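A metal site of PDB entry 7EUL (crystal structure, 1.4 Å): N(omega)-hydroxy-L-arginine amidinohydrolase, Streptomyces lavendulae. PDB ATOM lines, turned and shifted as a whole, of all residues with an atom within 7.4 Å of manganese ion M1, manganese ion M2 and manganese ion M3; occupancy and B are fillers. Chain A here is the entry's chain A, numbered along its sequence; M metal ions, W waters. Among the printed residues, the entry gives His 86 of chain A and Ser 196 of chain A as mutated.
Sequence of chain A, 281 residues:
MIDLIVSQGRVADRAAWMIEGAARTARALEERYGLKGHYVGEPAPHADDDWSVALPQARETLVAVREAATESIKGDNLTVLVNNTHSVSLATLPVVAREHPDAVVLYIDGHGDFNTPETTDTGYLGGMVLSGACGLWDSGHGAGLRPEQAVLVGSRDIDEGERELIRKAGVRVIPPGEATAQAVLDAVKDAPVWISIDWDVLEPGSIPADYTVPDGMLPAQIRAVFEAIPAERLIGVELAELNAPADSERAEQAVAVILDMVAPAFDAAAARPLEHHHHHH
A ring nitrogen (NE2) of His 86 sits at hydrogen-bond distance from the side-chain hydroxyl (OG) of Ser 196 (3.0 Å). The side-chain carboxylate of Asp 113 lies close to the side-chain hydroxyl of Tyr 107 (2.7 Å). The side-chain hydroxyl (OH) of Tyr 107 lies close to a ring nitrogen (NE2) of His 86. N of Val 129 is in hydrogen-bond range of O of Asp 113. N of Asp 198 sits at hydrogen-bond distance from O of Ile 108, 2.9 Å away. The side-chain carboxylate (OE2) of Glu 241 lies within hydrogen-bond range of the backbone NH (N) of His 86 (2.8 Å). OD1 of Asp 200 lies close to N of Gly 110, 3.0 Å away.
The nearest printed residue that does not touch manganese ion M1 is Tyr 107 (4.03 Å).
Manganese ion M3 is bound by water W4 (1.8 Å), the side-chain carboxylate (OD2) of Asp 200 (2.0 Å), the side-chain carboxylate (OD1) of Asp 200 (2.4 Å), the side-chain carboxylate (OD1) of Asp 109 (2.5 Å) and a ring nitrogen (ND1) of His 111 (2.5 Å). Slightly farther from manganese ion M3 lies the side-chain carboxylate (OD2) of Asp 198 (2.9 Å).
OD2 of Asp 109 is bound to manganese ion M1 (2.1 Å). Manganese ion M1 is bound by water W1, 2.2 Å away. The side-chain carboxylate (OD2) of Asp 113 is bound to manganese ion M1 (2.2 Å). Manganese ion M1 is bound by water W4 (2.3 Å). Manganese ion M1 is bound by ND1 of His 86 (2.3 Å). OD2 of Asp 198 is bound to manganese ion M1, at 2.3 Å.
Residues that only touch manganese ion M3: Gly 110 (3.996 Å). Five residues have an atom within 4 Å of manganese ion M3: Asp 109, Gly 110, His 111, Asp 198 and Asp 200. The nearest printed residue that does not touch manganese ion M3 is Asp 113 (4.2 Å).
Manganese ion M2 is bound by water W2 (1.9 Å), OE1 of Glu 241 (2.2 Å), OD2 of Asp 200 (2.3 Å), OD2 of Asp 198 (2.4 Å), water W3 (2.4 Å) and OD1 of Asp 198 (2.4 Å).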
ATOM      1  N   MET A  18      14.917  21.094 -16.085  1.00  0.00           N
ATOM      2  CA  MET A  18      15.188  19.938 -16.922  1.00  0.00           C
ATOM      3  C   MET A  18      15.150  18.630 -16.132  1.00  0.00           C
ATOM      4  O   MET A  18      14.773  17.604 -16.707  1.00  0.00           O
ATOM      5  CB  MET A  18      16.474  20.105 -17.729  1.00  0.00           C
ATOM      6  CG  MET A  18      16.233  20.763 -19.085  1.00  0.00           C
ATOM      7  SD  MET A  18      17.778  21.144 -19.923  1.00  0.00           S
ATOM      8  CE  MET A  18      18.643  21.855 -18.512  1.00  0.00           C
ATOM      9  N   THR A  85      19.674  16.396 -19.090  1.00  0.00           N
ATOM     10  CA  THR A  85      20.459  17.134 -20.072  1.00  0.00           C
ATOM     11  C   THR A  85      21.120  16.181 -21.060  1.00  0.00           C
ATOM     12  O   THR A  85      21.336  15.004 -20.775  1.00  0.00           O
ATOM     13  CB  THR A  85      21.565  17.978 -19.419  1.00  0.00           C
ATOM     14  OG1 THR A  85      22.539  17.115 -18.813  1.00  0.00           O
ATOM     15  CG2 THR A  85      20.996  18.923 -18.364  1.00  0.00           C
ATOM     16  N   HIS A  86      21.459  16.735 -22.226  1.00  0.00           N
ATOM     17  CA  HIS A  86      22.159  15.977 -23.262  1.00  0.00           C
ATOM     18  C   HIS A  86      23.547  15.540 -22.804  1.00  0.00           C
ATOM     19  O   HIS A  86      24.100  14.589 -23.367  1.00  0.00           O
ATOM     20  CB  HIS A  86      22.299  16.836 -24.507  1.00  0.00           C
ATOM     21  CG  HIS A  86      22.193  16.064 -25.782  1.00  0.00           C
ATOM     22  ND1 HIS A  86      22.064  16.687 -26.991  1.00  0.00           N
ATOM     23  CD2 HIS A  86      22.186  14.731 -26.013  1.00  0.00           C
ATOM     24  CE1 HIS A  86      21.930  15.762 -27.941  1.00  0.00           C
ATOM     25  NE2 HIS A  86      22.046  14.575 -27.378  1.00  0.00           N
ATOM     26  N   SER A  87      24.121  16.232 -21.814  1.00  0.00           N
ATOM     27  CA  SER A  87      25.458  15.882 -21.324  1.00  0.00           C
ATOM     28  C   SER A  87      25.513  14.484 -20.704  1.00  0.00           C
ATOM     29  O   SER A  87      26.599  13.919 -20.622  1.00  0.00           O
ATOM     30  CB  SER A  87      25.939  16.935 -20.334  1.00  0.00           C
ATOM     31  OG  SER A  87      26.130  18.197 -20.988  1.00  0.00           O
ATOM     32  N   TYR A 107      22.257  11.744 -34.101  1.00  0.00           N
ATOM     33  CA  TYR A 107      22.354  12.772 -33.062  1.00  0.00           C
ATOM     34  C   TYR A 107      21.444  13.929 -33.496  1.00  0.00           C
ATOM     35  O   TYR A 107      21.809  14.745 -34.340  1.00  0.00           O
ATOM     36  CB  TYR A 107      23.803  13.179 -32.894  1.00  0.00           C
ATOM     37  CG  TYR A 107      24.133  13.919 -31.615  1.00  0.00           C
ATOM     38  CD1 TYR A 107      23.991  15.305 -31.541  1.00  0.00           C
ATOM     39  CD2 TYR A 107      24.630  13.248 -30.503  1.00  0.00           C
ATOM     40  CE1 TYR A 107      24.300  16.001 -30.359  1.00  0.00           C
ATOM     41  CE2 TYR A 107      24.939  13.938 -29.333  1.00  0.00           C
ATOM     42  CZ  TYR A 107      24.785  15.309 -29.266  1.00  0.00           C
ATOM     43  OH  TYR A 107      25.094  15.991 -28.109  1.00  0.00           O
ATOM     44  N   ILE A 108      20.233  13.947 -32.960  1.00  0.00           N
ATOM     45  CA  ILE A 108      19.167  14.801 -33.469  1.00  0.00           C
ATOM     46  C   ILE A 108      19.117  16.017 -32.567  1.00  0.00           C
ATOM     47  O   ILE A 108      18.724  15.912 -31.396  1.00  0.00           O
ATOM     48  CB  ILE A 108      17.838  14.034 -33.516  1.00  0.00           C
ATOM     49  CG1 ILE A 108      18.022  12.714 -34.298  1.00  0.00           C
ATOM     50  CG2 ILE A 108      16.744  14.908 -34.158  1.00  0.00           C
ATOM     51  CD1 ILE A 108      16.728  11.930 -34.523  1.00  0.00           C
ATOM     52  N   ASP A 109      19.524  17.168 -33.098  1.00  0.00           N
ATOM     53  CA  ASP A 109      19.907  18.285 -32.257  1.00  0.00           C
ATOM     54  C   ASP A 109      19.887  19.560 -33.084  1.00  0.00           C
ATOM     55  O   ASP A 109      20.291  19.545 -34.243  1.00  0.00           O
ATOM     56  CB  ASP A 109      21.331  18.042 -31.732  1.00  0.00           C
ATOM     57  CG  ASP A 109      21.675  18.890 -30.532  1.00  0.00           C
ATOM     58  OD1 ASP A 109      21.793  20.114 -30.649  1.00  0.00           O
ATOM     59  OD2 ASP A 109      21.790  18.323 -29.444  1.00  0.00           O
ATOM     60  N   GLY A 110      19.470  20.671 -32.478  1.00  0.00           N
ATOM     61  CA  GLY A 110      19.512  21.942 -33.174  1.00  0.00           C
ATOM     62  C   GLY A 110      20.905  22.525 -33.333  1.00  0.00           C
ATOM     63  O   GLY A 110      21.114  23.400 -34.174  1.00  0.00           O
ATOM     64  N   HIS A 111      21.856  22.035 -32.557  1.00  0.00           N
ATOM     65  CA  HIS A 111      23.239  22.460 -32.544  1.00  0.00           C
ATOM     66  C   HIS A 111      24.114  21.264 -32.951  1.00  0.00           C
ATOM     67  O   HIS A 111      23.614  20.154 -33.174  1.00  0.00           O
ATOM     68  CB  HIS A 111      23.612  22.933 -31.138  1.00  0.00           C
ATOM     69  CG  HIS A 111      22.694  23.989 -30.601  1.00  0.00           C
ATOM     70  ND1 HIS A 111      21.609  23.696 -29.809  1.00  0.00           N
ATOM     71  CD2 HIS A 111      22.714  25.333 -30.735  1.00  0.00           C
ATOM     72  CE1 HIS A 111      20.978  24.820 -29.482  1.00  0.00           C
ATOM     73  NE2 HIS A 111      21.633  25.828 -30.036  1.00  0.00           N
ATOM     74  N   GLY A 112      25.405  21.490 -33.074  1.00  0.00           N
ATOM     75  CA  GLY A 112      26.266  20.363 -33.357  1.00  0.00           C
ATOM     76  C   GLY A 112      26.881  19.701 -32.139  1.00  0.00           C
ATOM     77  O   GLY A 112      27.400  18.581 -32.253  1.00  0.00           O
ATOM     78  N   ASP A 113      26.825  20.368 -30.979  1.00  0.00           N
ATOM     79  CA  ASP A 113      27.449  19.870 -29.757  1.00  0.00           C
ATOM     80  C   ASP A 113      28.873  19.356 -30.007  1.00  0.00           C
ATOM     81  O   ASP A 113      29.281  18.328 -29.470  1.00  0.00           O
ATOM     82  CB  ASP A 113      26.575  18.822 -29.068  1.00  0.00           C
ATOM     83  CG  ASP A 113      25.244  19.384 -28.621  1.00  0.00           C
ATOM     84  OD1 ASP A 113      25.019  20.616 -28.733  1.00  0.00           O
ATOM     85  OD2 ASP A 113      24.427  18.591 -28.128  1.00  0.00           O
ATOM     86  N   TYR A 124      30.026  25.749 -21.855  1.00  0.00           N
ATOM     87  CA  TYR A 124      28.882  24.895 -21.539  1.00  0.00           C
ATOM     88  C   TYR A 124      29.143  23.451 -21.967  1.00  0.00           C
ATOM     89  O   TYR A 124      29.357  23.172 -23.150  1.00  0.00           O
ATOM     90  CB  TYR A 124      27.605  25.428 -22.193  1.00  0.00           C
ATOM     91  CG  TYR A 124      26.409  24.555 -21.897  1.00  0.00           C
ATOM     92  CD1 TYR A 124      26.189  24.080 -20.609  1.00  0.00           C
ATOM     93  CD2 TYR A 124      25.511  24.185 -22.900  1.00  0.00           C
ATOM     94  CE1 TYR A 124      25.115  23.267 -20.318  1.00  0.00           C
ATOM     95  CE2 TYR A 124      24.437  23.365 -22.622  1.00  0.00           C
ATOM     96  CZ  TYR A 124      24.244  22.921 -21.327  1.00  0.00           C
ATOM     97  OH  TYR A 124      23.171  22.094 -21.037  1.00  0.00           O
ATOM     98  N   GLY A 126      27.158  21.015 -22.361  1.00  0.00           N
ATOM     99  CA  GLY A 126      26.206  20.492 -23.323  1.00  0.00           C
ATOM    100  C   GLY A 126      26.571  20.767 -24.770  1.00  0.00           C
ATOM    101  O   GLY A 126      26.066  20.088 -25.671  1.00  0.00           O
ATOM    102  N   GLY A 127      27.425  21.753 -25.007  1.00  0.00           N
ATOM    103  CA  GLY A 127      27.920  22.024 -26.341  1.00  0.00           C
ATOM    104  C   GLY A 127      29.145  21.247 -26.736  1.00  0.00           C
ATOM    105  O   GLY A 127      29.707  21.514 -27.808  1.00  0.00           O
ATOM    106  N   VAL A 129      29.281  17.579 -26.196  1.00  0.00           N
ATOM    107  CA  VAL A 129      28.925  16.179 -25.964  1.00  0.00           C
ATOM    108  C   VAL A 129      29.404  15.269 -27.094  1.00  0.00           C
ATOM    109  O   VAL A 129      30.013  14.223 -26.846  1.00  0.00           O
ATOM    110  CB  VAL A 129      27.404  16.068 -25.762  1.00  0.00           C
ATOM    111  CG1 VAL A 129      27.005  14.629 -25.604  1.00  0.00           C
ATOM    112  CG2 VAL A 129      26.949  16.887 -24.564  1.00  0.00           C
ATOM    113  N   SER A 196      19.731   9.714 -30.361  1.00  0.00           N
ATOM    114  CA  SER A 196      19.889  10.640 -29.232  1.00  0.00           C
ATOM    115  C   SER A 196      19.276  11.970 -29.618  1.00  0.00           C
ATOM    116  O   SER A 196      19.770  12.627 -30.546  1.00  0.00           O
ATOM    117  CB  SER A 196      21.368  10.829 -28.907  1.00  0.00           C
ATOM    118  OG  SER A 196      21.541  11.657 -27.764  1.00  0.00           O
ATOM    119  N   ILE A 197      18.213  12.389 -28.925  1.00  0.00           N
ATOM    120  CA  ILE A 197      17.417  13.548 -29.290  1.00  0.00           C
ATOM    121  C   ILE A 197      17.548  14.635 -28.204  1.00  0.00           C
ATOM    122  O   ILE A 197      17.411  14.324 -27.020  1.00  0.00           O
ATOM    123  CB  ILE A 197      15.931  13.187 -29.443  1.00  0.00           C
ATOM    124  CG1 ILE A 197      15.718  12.286 -30.649  1.00  0.00           C
ATOM    125  CG2 ILE A 197      15.076  14.453 -29.557  1.00  0.00           C
ATOM    126  CD1 ILE A 197      14.324  11.719 -30.735  1.00  0.00           C
ATOM    127  N   ASP A 198      17.763  15.876 -28.635  1.00  0.00           N
ATOM    128  CA  ASP A 198      17.697  17.085 -27.801  1.00  0.00           C
ATOM    129  C   ASP A 198      16.517  17.873 -28.359  1.00  0.00           C
ATOM    130  O   ASP A 198      16.518  18.209 -29.554  1.00  0.00           O
ATOM    131  CB  ASP A 198      19.008  17.852 -27.999  1.00  0.00           C
ATOM    132  CG  ASP A 198      19.112  19.146 -27.210  1.00  0.00           C
ATOM    133  OD1 ASP A 198      18.091  19.806 -26.933  1.00  0.00           O
ATOM    134  OD2 ASP A 198      20.243  19.540 -26.871  1.00  0.00           O
ATOM    135  N   TRP A 199      15.510  18.154 -27.523  1.00  0.00           N
ATOM    136  CA  TRP A 199      14.287  18.810 -28.021  1.00  0.00           C
ATOM    137  C   TRP A 199      14.508  20.209 -28.591  1.00  0.00           C
ATOM    138  O   TRP A 199      13.593  20.729 -29.239  1.00  0.00           O
ATOM    139  CB  TRP A 199      13.161  18.824 -26.980  1.00  0.00           C
ATOM    140  CG  TRP A 199      12.766  17.448 -26.523  1.00  0.00           C
ATOM    141  CD1 TRP A 199      12.800  16.979 -25.245  1.00  0.00           C
ATOM    142  CD2 TRP A 199      12.302  16.353 -27.343  1.00  0.00           C
ATOM    143  NE1 TRP A 199      12.381  15.668 -25.209  1.00  0.00           N
ATOM    144  CE2 TRP A 199      12.077  15.263 -26.477  1.00  0.00           C
ATOM    145  CE3 TRP A 199      12.062  16.202 -28.709  1.00  0.00           C
ATOM    146  CZ2 TRP A 199      11.610  14.030 -26.932  1.00  0.00           C
ATOM    147  CZ3 TRP A 199      11.607  14.963 -29.169  1.00  0.00           C
ATOM    148  CH2 TRP A 199      11.388  13.895 -28.275  1.00  0.00           C
ATOM    149  N   ASP A 200      15.691  20.822 -28.420  1.00  0.00           N
ATOM    150  CA  ASP A 200      15.936  22.075 -29.135  1.00  0.00           C
ATOM    151  C   ASP A 200      16.061  21.891 -30.647  1.00  0.00           C
ATOM    152  O   ASP A 200      16.181  22.885 -31.383  1.00  0.00           O
ATOM    153  CB  ASP A 200      17.124  22.861 -28.542  1.00  0.00           C
ATOM    154  CG  ASP A 200      18.484  22.179 -28.734  1.00  0.00           C
ATOM    155  OD1 ASP A 200      18.691  21.451 -29.725  1.00  0.00           O
ATOM    156  OD2 ASP A 200      19.365  22.407 -27.878  1.00  0.00           O
ATOM    157  N   VAL A 201      16.027  20.643 -31.147  1.00  0.00           N
ATOM    158  CA  VAL A 201      15.980  20.417 -32.589  1.00  0.00           C
ATOM    159  C   VAL A 201      14.673  20.933 -33.191  1.00  0.00           C
ATOM    160  O   VAL A 201      14.623  21.272 -34.370  1.00  0.00           O
ATOM    161  CB  VAL A 201      16.222  18.935 -32.912  1.00  0.00           C
ATOM    162  CG1 VAL A 201      14.989  18.080 -32.544  1.00  0.00           C
ATOM    163  CG2 VAL A 201      16.586  18.778 -34.372  1.00  0.00           C
ATOM    164  N   ALA A 209      12.645  23.799 -24.369  1.00  0.00           N
ATOM    165  CA  ALA A 209      13.960  23.237 -24.091  1.00  0.00           C
ATOM    166  C   ALA A 209      14.837  24.310 -23.458  1.00  0.00           C
ATOM    167  O   ALA A 209      14.326  25.236 -22.825  1.00  0.00           O
ATOM    168  CB  ALA A 209      14.587  22.652 -25.371  1.00  0.00           C
ATOM    169  N   ASP A 210      16.155  24.191 -23.596  1.00  0.00           N
ATOM    170  CA  ASP A 210      17.036  25.209 -23.046  1.00  0.00           C
ATOM    171  C   ASP A 210      17.342  26.292 -24.073  1.00  0.00           C
ATOM    172  O   ASP A 210      17.362  27.483 -23.737  1.00  0.00           O
ATOM    173  CB  ASP A 210      18.340  24.559 -22.546  1.00  0.00           C
ATOM    174  CG  ASP A 210      19.151  25.476 -21.634  1.00  0.00           C
ATOM    175  OD1 ASP A 210      18.717  26.609 -21.374  1.00  0.00           O
ATOM    176  OD2 ASP A 210      20.226  25.027 -21.178  1.00  0.00           O
ATOM    177  N   TYR A 211      17.555  25.900 -25.322  1.00  0.00           N
ATOM    178  CA  TYR A 211      17.884  26.822 -26.380  1.00  0.00           C
ATOM    179  C   TYR A 211      16.770  26.875 -27.407  1.00  0.00           C
ATOM    180  O   TYR A 211      15.958  25.952 -27.549  1.00  0.00           O
ATOM    181  CB  TYR A 211      19.213  26.446 -27.040  1.00  0.00           C
ATOM    182  CG  TYR A 211      20.379  26.668 -26.106  1.00  0.00           C
ATOM    183  CD1 TYR A 211      20.680  25.733 -25.115  1.00  0.00           C
ATOM    184  CD2 TYR A 211      21.145  27.823 -26.177  1.00  0.00           C
ATOM    185  CE1 TYR A 211      21.733  25.933 -24.239  1.00  0.00           C
ATOM    186  CE2 TYR A 211      22.197  28.029 -25.313  1.00  0.00           C
ATOM    187  CZ  TYR A 211      22.485  27.087 -24.341  1.00  0.00           C
ATOM    188  OH  TYR A 211      23.537  27.293 -23.477  1.00  0.00           O
ATOM    189  N   VAL A 213      16.454  27.688 -31.263  1.00  0.00           N
ATOM    190  CA  VAL A 213      17.050  27.875 -32.576  1.00  0.00           C
ATOM    191  C   VAL A 213      15.916  27.968 -33.601  1.00  0.00           C
ATOM    192  O   VAL A 213      15.143  27.006 -33.722  1.00  0.00           O
ATOM    193  CB  VAL A 213      18.001  26.727 -32.922  1.00  0.00           C
ATOM    194  CG1 VAL A 213      18.955  27.154 -34.007  1.00  0.00           C
ATOM    195  CG2 VAL A 213      18.763  26.276 -31.674  1.00  0.00           C
ATOM    196  N   ALA A 240      16.185  13.990 -24.318  1.00  0.00           N
ATOM    197  CA  ALA A 240      16.806  14.956 -23.413  1.00  0.00           C
ATOM    198  C   ALA A 240      16.281  16.362 -23.625  1.00  0.00           C
ATOM    199  O   ALA A 240      15.967  16.771 -24.747  1.00  0.00           O
ATOM    200  CB  ALA A 240      18.333  14.996 -23.615  1.00  0.00           C
ATOM    201  N   GLU A 241      16.215  17.100 -22.513  1.00  0.00           N
ATOM    202  CA  GLU A 241      16.089  18.551 -22.460  1.00  0.00           C
ATOM    203  C   GLU A 241      14.676  19.090 -22.600  1.00  0.00           C
ATOM    204  O   GLU A 241      14.445  20.105 -23.265  1.00  0.00           O
ATOM    205  CB  GLU A 241      17.066  19.241 -23.411  1.00  0.00           C
ATOM    206  CG  GLU A 241      18.473  18.666 -23.324  1.00  0.00           C
ATOM    207  CD  GLU A 241      19.534  19.716 -23.212  1.00  0.00           C
ATOM    208  OE1 GLU A 241      19.304  20.843 -23.672  1.00  0.00           O
ATOM    209  OE2 GLU A 241      20.622  19.402 -22.671  1.00  0.00           O
HETATM  210 MN    MN M   1      22.349  18.878 -27.479  1.00  0.00          MN
HETATM  211 MN    MN M   2      19.375  21.440 -25.743  1.00  0.00          MN
HETATM  212 MN    MN M   3      20.915  21.533 -28.853  1.00  0.00          MN
HETATM  213  O   HOH W   1      23.315  19.538 -25.625  1.00  0.00           O
HETATM  214  O   HOH W   2      18.297  22.902 -25.198  1.00  0.00           O
HETATM  215  O   HOH W   3      21.605  22.229 -25.505  1.00  0.00           O
HETATM  216  O   HOH W   4      22.437  21.054 -28.050  1.00  0.00           O
